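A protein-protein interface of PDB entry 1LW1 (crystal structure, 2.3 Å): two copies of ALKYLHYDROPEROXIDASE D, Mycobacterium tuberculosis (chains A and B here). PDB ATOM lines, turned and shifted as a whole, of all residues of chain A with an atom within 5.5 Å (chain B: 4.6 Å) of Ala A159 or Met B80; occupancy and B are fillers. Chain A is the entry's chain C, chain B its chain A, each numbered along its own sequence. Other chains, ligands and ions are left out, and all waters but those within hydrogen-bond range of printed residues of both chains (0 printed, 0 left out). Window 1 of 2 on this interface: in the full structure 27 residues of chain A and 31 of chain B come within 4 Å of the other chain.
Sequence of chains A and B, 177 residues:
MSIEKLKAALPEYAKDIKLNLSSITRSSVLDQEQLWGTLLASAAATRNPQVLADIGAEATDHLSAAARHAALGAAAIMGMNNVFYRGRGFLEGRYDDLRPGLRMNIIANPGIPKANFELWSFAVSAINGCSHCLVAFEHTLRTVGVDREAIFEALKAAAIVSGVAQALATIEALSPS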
ATOM      1  N   ASN A  20      12.735  14.415  32.616  1.00  0.00           N
ATOM      2  CA  ASN A  20      12.386  13.437  31.593  1.00  0.00           C
ATOM      3  C   ASN A  20      11.825  12.198  32.304  1.00  0.00           C
ATOM      4  O   ASN A  20      10.856  11.593  31.858  1.00  0.00           O
ATOM      5  CB  ASN A  20      13.634  13.057  30.765  1.00  0.00           C
ATOM      6  CG  ASN A  20      14.055  14.149  29.771  1.00  0.00           C
ATOM      7  OD1 ASN A  20      15.240  14.302  29.464  1.00  0.00           O
ATOM      8  ND2 ASN A  20      13.081  14.899  29.258  1.00  0.00           N
ATOM      9  N   ILE A 127      19.437   0.003  24.359  1.00  0.00           N
ATOM     10  CA  ILE A 127      20.440   0.331  25.362  1.00  0.00           C
ATOM     11  C   ILE A 127      21.765  -0.356  25.064  1.00  0.00           C
ATOM     12  O   ILE A 127      22.825   0.271  25.078  1.00  0.00           O
ATOM     13  CB  ILE A 127      19.954  -0.046  26.792  1.00  0.00           C
ATOM     14  CG1 ILE A 127      18.782   0.855  27.206  1.00  0.00           C
ATOM     15  CG2 ILE A 127      21.105   0.106  27.778  1.00  0.00           C
ATOM     16  CD1 ILE A 127      17.895   0.288  28.309  1.00  0.00           C
ATOM     17  N   ALA A 154       8.911   3.693  23.779  1.00  0.00           N
ATOM     18  CA  ALA A 154       9.770   2.697  24.397  1.00  0.00           C
ATOM     19  C   ALA A 154      11.235   3.123  24.209  1.00  0.00           C
ATOM     20  O   ALA A 154      12.071   2.972  25.109  1.00  0.00           O
ATOM     21  CB  ALA A 154       9.525   1.332  23.764  1.00  0.00           C
ATOM     22  N   LEU A 155      11.531   3.666  23.036  1.00  0.00           N
ATOM     23  CA  LEU A 155      12.873   4.119  22.738  1.00  0.00           C
ATOM     24  C   LEU A 155      13.244   5.245  23.680  1.00  0.00           C
ATOM     25  O   LEU A 155      14.352   5.283  24.212  1.00  0.00           O
ATOM     26  CB  LEU A 155      12.960   4.621  21.302  1.00  0.00           C
ATOM     27  CG  LEU A 155      14.280   5.308  20.961  1.00  0.00           C
ATOM     28  CD1 LEU A 155      15.489   4.475  21.444  1.00  0.00           C
ATOM     29  CD2 LEU A 155      14.332   5.494  19.481  1.00  0.00           C
ATOM     30  N   LYS A 156      12.305   6.165  23.870  1.00  0.00           N
ATOM     31  CA  LYS A 156      12.521   7.315  24.734  1.00  0.00           C
ATOM     32  C   LYS A 156      12.732   6.831  26.161  1.00  0.00           C
ATOM     33  O   LYS A 156      13.633   7.303  26.867  1.00  0.00           O
ATOM     34  CB  LYS A 156      11.317   8.249  24.666  1.00  0.00           C
ATOM     35  CG  LYS A 156      11.239   9.067  23.380  1.00  0.00           C
ATOM     36  CD  LYS A 156       9.895   9.740  23.234  1.00  0.00           C
ATOM     37  CE  LYS A 156       9.627  10.729  24.353  1.00  0.00           C
ATOM     38  NZ  LYS A 156       8.212  11.196  24.328  1.00  0.00           N
ATOM     39  N   ALA A 157      11.901   5.869  26.556  1.00  0.00           N
ATOM     40  CA  ALA A 157      11.947   5.280  27.887  1.00  0.00           C
ATOM     41  C   ALA A 157      13.290   4.607  28.129  1.00  0.00           C
ATOM     42  O   ALA A 157      13.846   4.692  29.212  1.00  0.00           O
ATOM     43  CB  ALA A 157      10.822   4.267  28.043  1.00  0.00           C
ATOM     44  N   ALA A 158      13.813   3.949  27.108  1.00  0.00           N
ATOM     45  CA  ALA A 158      15.088   3.266  27.225  1.00  0.00           C
ATOM     46  C   ALA A 158      16.182   4.281  27.458  1.00  0.00           C
ATOM     47  O   ALA A 158      17.067   4.077  28.286  1.00  0.00           O
ATOM     48  CB  ALA A 158      15.383   2.451  25.956  1.00  0.00           C
ATOM     49  N   ALA A 159      16.117   5.378  26.718  1.00  0.00           N
ATOM     50  CA  ALA A 159      17.105   6.433  26.840  1.00  0.00           C
ATOM     51  C   ALA A 159      16.987   7.204  28.161  1.00  0.00           C
ATOM     52  O   ALA A 159      17.991   7.459  28.808  1.00  0.00           O
ATOM     53  CB  ALA A 159      16.992   7.395  25.647  1.00  0.00           C
ATOM     54  N   ILE A 160      15.779   7.581  28.573  1.00  0.00           N
ATOM     55  CA  ILE A 160      15.671   8.327  29.827  1.00  0.00           C
ATOM     56  C   ILE A 160      16.300   7.513  30.967  1.00  0.00           C
ATOM     57  O   ILE A 160      17.114   8.022  31.730  1.00  0.00           O
ATOM     58  CB  ILE A 160      14.193   8.671  30.141  1.00  0.00           C
ATOM     59  CG1 ILE A 160      13.666   9.628  29.072  1.00  0.00           C
ATOM     60  CG2 ILE A 160      14.076   9.377  31.498  1.00  0.00           C
ATOM     61  CD1 ILE A 160      12.177   9.807  29.055  1.00  0.00           C
ATOM     62  N   VAL A 161      15.931   6.242  31.056  1.00  0.00           N
ATOM     63  CA  VAL A 161      16.447   5.345  32.076  1.00  0.00           C
ATOM     64  C   VAL A 161      17.965   5.160  32.017  1.00  0.00           C
ATOM     65  O   VAL A 161      18.607   4.913  33.037  1.00  0.00           O
ATOM     66  CB  VAL A 161      15.749   3.977  31.979  1.00  0.00           C
ATOM     67  CG1 VAL A 161      16.450   2.956  32.851  1.00  0.00           C
ATOM     68  CG2 VAL A 161      14.308   4.120  32.401  1.00  0.00           C
ATOM     69  N   SER A 162      18.546   5.283  30.829  1.00  0.00           N
ATOM     70  CA  SER A 162      19.995   5.148  30.697  1.00  0.00           C
ATOM     71  C   SER A 162      20.658   6.366  31.331  1.00  0.00           C
ATOM     72  O   SER A 162      21.684   6.242  31.998  1.00  0.00           O
ATOM     73  CB  SER A 162      20.400   5.052  29.221  1.00  0.00           C
ATOM     74  OG  SER A 162      19.974   3.818  28.667  1.00  0.00           O
ATOM     75  N   GLY A 163      20.066   7.538  31.100  1.00  0.00           N
ATOM     76  CA  GLY A 163      20.580   8.769  31.669  1.00  0.00           C
ATOM     77  C   GLY A 163      20.423   8.748  33.180  1.00  0.00           C
ATOM     78  O   GLY A 163      21.327   9.156  33.914  1.00  0.00           O
ATOM     79  N   VAL A 164      19.274   8.261  33.643  1.00  0.00           N
ATOM     80  CA  VAL A 164      18.995   8.164  35.060  1.00  0.00           C
ATOM     81  C   VAL A 164      20.114   7.363  35.706  1.00  0.00           C
ATOM     82  O   VAL A 164      20.832   7.853  36.582  1.00  0.00           O
ATOM     83  CB  VAL A 164      17.655   7.472  35.303  1.00  0.00           C
ATOM     84  CG1 VAL A 164      17.532   7.077  36.786  1.00  0.00           C
ATOM     85  CG2 VAL A 164      16.510   8.410  34.908  1.00  0.00           C
ATOM     86  N   ALA B  76      25.960  12.615  31.997  1.00  0.00           N
ATOM     87  CA  ALA B  76      24.575  12.330  32.303  1.00  0.00           C
ATOM     88  C   ALA B  76      23.680  12.500  31.079  1.00  0.00           C
ATOM     89  O   ALA B  76      23.000  11.555  30.688  1.00  0.00           O
ATOM     90  CB  ALA B  76      24.099  13.220  33.422  1.00  0.00           C
ATOM     91  N   ILE B  77      23.653  13.683  30.467  1.00  0.00           N
ATOM     92  CA  ILE B  77      22.772  13.821  29.315  1.00  0.00           C
ATOM     93  C   ILE B  77      23.188  12.981  28.115  1.00  0.00           C
ATOM     94  O   ILE B  77      22.336  12.603  27.296  1.00  0.00           O
ATOM     95  CB  ILE B  77      22.599  15.294  28.842  1.00  0.00           C
ATOM     96  CG1 ILE B  77      23.897  16.070  29.019  1.00  0.00           C
ATOM     97  CG2 ILE B  77      21.409  15.919  29.543  1.00  0.00           C
ATOM     98  CD1 ILE B  77      24.934  15.773  27.974  1.00  0.00           C
ATOM     99  N   MET B  78      24.481  12.689  28.002  1.00  0.00           N
ATOM    100  CA  MET B  78      24.939  11.890  26.884  1.00  0.00           C
ATOM    101  C   MET B  78      24.481  10.443  27.106  1.00  0.00           C
ATOM    102  O   MET B  78      24.237   9.702  26.154  1.00  0.00           O
ATOM    103  CB  MET B  78      26.456  12.011  26.740  1.00  0.00           C
ATOM    104  CG  MET B  78      26.923  12.520  25.362  1.00  0.00           C
ATOM    105  SD  MET B  78      25.964  13.898  24.617  1.00  0.00           S
ATOM    106  CE  MET B  78      25.009  13.064  23.476  1.00  0.00           C
ATOM    107  N   GLY B  79      24.319  10.056  28.369  1.00  0.00           N
ATOM    108  CA  GLY B  79      23.863   8.710  28.680  1.00  0.00           C
ATOM    109  C   GLY B  79      22.466   8.472  28.143  1.00  0.00           C
ATOM    110  O   GLY B  79      22.067   7.337  27.854  1.00  0.00           O
ATOM    111  N   MET B  80      21.701   9.547  28.016  1.00  0.00           N
ATOM    112  CA  MET B  80      20.357   9.439  27.468  1.00  0.00           C
ATOM    113  C   MET B  80      20.438   9.545  25.921  1.00  0.00           C
ATOM    114  O   MET B  80      20.088   8.604  25.197  1.00  0.00           O
ATOM    115  CB  MET B  80      19.463  10.554  28.035  1.00  0.00           C
ATOM    116  CG  MET B  80      18.072  10.623  27.398  1.00  0.00           C
ATOM    117  SD  MET B  80      16.990  11.925  28.065  1.00  0.00           S
ATOM    118  CE  MET B  80      17.818  13.423  27.479  1.00  0.00           C
ATOM    119  N   ASN B  81      20.921  10.694  25.450  1.00  0.00           N
ATOM    120  CA  ASN B  81      21.067  11.024  24.034  1.00  0.00           C
ATOM    121  C   ASN B  81      21.770   9.950  23.209  1.00  0.00           C
ATOM    122  O   ASN B  81      21.348   9.635  22.097  1.00  0.00           O
ATOM    123  CB  ASN B  81      21.830  12.351  23.899  1.00  0.00           C
ATOM    124  CG  ASN B  81      20.972  13.556  24.221  1.00  0.00           C
ATOM    125  OD1 ASN B  81      19.899  13.434  24.812  1.00  0.00           O
ATOM    126  ND2 ASN B  81      21.444  14.734  23.832  1.00  0.00           N
ATOM    127  N   ASN B  82      22.855   9.400  23.747  1.00  0.00           N
ATOM    128  CA  ASN B  82      23.606   8.369  23.041  1.00  0.00           C
ATOM    129  C   ASN B  82      22.767   7.108  22.767  1.00  0.00           C
ATOM    130  O   ASN B  82      23.057   6.349  21.839  1.00  0.00           O
ATOM    131  CB  ASN B  82      24.862   7.995  23.836  1.00  0.00           C
ATOM    132  CG  ASN B  82      25.949   9.045  23.747  1.00  0.00           C
ATOM    133  OD1 ASN B  82      26.966   8.957  24.445  1.00  0.00           O
ATOM    134  ND2 ASN B  82      25.752  10.041  22.889  1.00  0.00           N
ATOM    135  N   VAL B  83      21.747   6.870  23.592  1.00  0.00           N
ATOM    136  CA  VAL B  83      20.882   5.710  23.407  1.00  0.00           C
ATOM    137  C   VAL B  83      19.774   6.108  22.431  1.00  0.00           C
ATOM    138  O   VAL B  83      19.378   5.325  21.565  1.00  0.00           O
ATOM    139  CB  VAL B  83      20.236   5.223  24.775  1.00  0.00           C
ATOM    140  CG1 VAL B  83      19.119   4.223  24.517  1.00  0.00           C
ATOM    141  CG2 VAL B  83      21.282   4.535  25.651  1.00  0.00           C
ATOM    142  N   PHE B  84      19.287   7.337  22.564  1.00  0.00           N
ATOM    143  CA  PHE B  84      18.208   7.805  21.713  1.00  0.00           C
ATOM    144  C   PHE B  84      18.577   7.956  20.243  1.00  0.00           C
ATOM    145  O   PHE B  84      18.012   7.297  19.388  1.00  0.00           O
ATOM    146  CB  PHE B  84      17.670   9.141  22.219  1.00  0.00           C
ATOM    147  CG  PHE B  84      16.461   9.616  21.467  1.00  0.00           C
ATOM    148  CD1 PHE B  84      15.246   8.969  21.608  1.00  0.00           C
ATOM    149  CD2 PHE B  84      16.544  10.701  20.602  1.00  0.00           C
ATOM    150  CE1 PHE B  84      14.131   9.394  20.905  1.00  0.00           C
ATOM    151  CE2 PHE B  84      15.430  11.133  19.894  1.00  0.00           C
ATOM    152  CZ  PHE B  84      14.225  10.477  20.047  1.00  0.00           C
ATOM    153  N   LEU B 102      12.414  15.249  24.564  1.00  0.00           N
ATOM    154  CA  LEU B 102      13.352  15.050  25.659  1.00  0.00           C
ATOM    155  C   LEU B 102      13.997  16.345  26.124  1.00  0.00           C
ATOM    156  O   LEU B 102      14.472  17.136  25.315  1.00  0.00           O
ATOM    157  CB  LEU B 102      14.446  14.074  25.233  1.00  0.00           C
ATOM    158  CG  LEU B 102      13.915  12.711  24.809  1.00  0.00           C
ATOM    159  CD1 LEU B 102      15.075  11.795  24.411  1.00  0.00           C
ATOM    160  CD2 LEU B 102      13.128  12.129  25.957  1.00  0.00           C
ATOM    161  N   ARG B 103      14.007  16.549  27.435  1.00  0.00           N
ATOM    162  CA  ARG B 103      14.612  17.726  28.033  1.00  0.00           C
ATOM    163  C   ARG B 103      16.135  17.594  27.933  1.00  0.00           C
ATOM    164  O   ARG B 103      16.687  16.510  28.150  1.00  0.00           O
ATOM    165  CB  ARG B 103      14.211  17.816  29.505  1.00  0.00           C
ATOM    166  CG  ARG B 103      13.212  18.897  29.851  1.00  0.00           C
ATOM    167  CD  ARG B 103      13.774  20.284  29.581  1.00  0.00           C
ATOM    168  NE  ARG B 103      13.465  21.218  30.663  1.00  0.00           N
ATOM    169  CZ  ARG B 103      14.198  21.358  31.764  1.00  0.00           C
ATOM    170  NH1 ARG B 103      15.293  20.628  31.934  1.00  0.00           N
ATOM    171  NH2 ARG B 103      13.834  22.222  32.702  1.00  0.00           N
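SD of Met B80 sits close to OD1 of Asn A20 (3.3 Å).
The side-chain amide nitrogen (ND2) of Asn A20 lies close to the backbone NH (N) of Arg B103 (2.6 Å).
OG of Ser A162 is in hydrogen-bond range of O of Ala A158, 2.9 Å away.
Among the printed residues, pairs that only touch across the chains: Ser A162 with Gly B79, Ala A159 with Met B80, Ser A162 with Val B83, Asn A20 with Leu B102, Ala A159 with Val B83, Gly A163 with Ala B76, Gly A163 with Gly B79, Lys A156 with Phe B84, Leu A155 with Phe B84, Ala A159 with Phe B84, Gly A163 with Met B80, Leu A155 with Val B83, Ile A160 with Met B80 and Ile A160 with Leu B102.
No position is printed for both chains.
Ala A154 touches none of the printed residues of chain B.
Printed residues of chain B within 4 Å of Lys A156: Phe B84 (3.8 Å).
Ala A159 touches three residues of chain B.
Of the printed residues of chain A, Ala B76 touches Gly A163.
Printed residues of chain A within 4 Å of Met B80: Asn A20 (3.3 Å), Ala A159 (3.4 Å), Ile A160 (3.99 Å) and Gly A163 (3.9 Å).
The nearest residue of chain B that does not touch Ala A159 is Gly B79 (4.2 Å).
The nearest printed residue of chain A that does not touch Met B80 is Ser A162 (4.7 Å).
Of the 13 printed residues of chain A, 7 touch a printed residue of chain B.
Hydrophobic or aromatic side chains of chain A that line the printed part of chain B: Leu A155, Ala A159 and Ile A160.
Of the 11 printed residues of chain B, 7 touch a printed residue of chain A.
Among the printed residues, 16 pairs touch across the chains.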
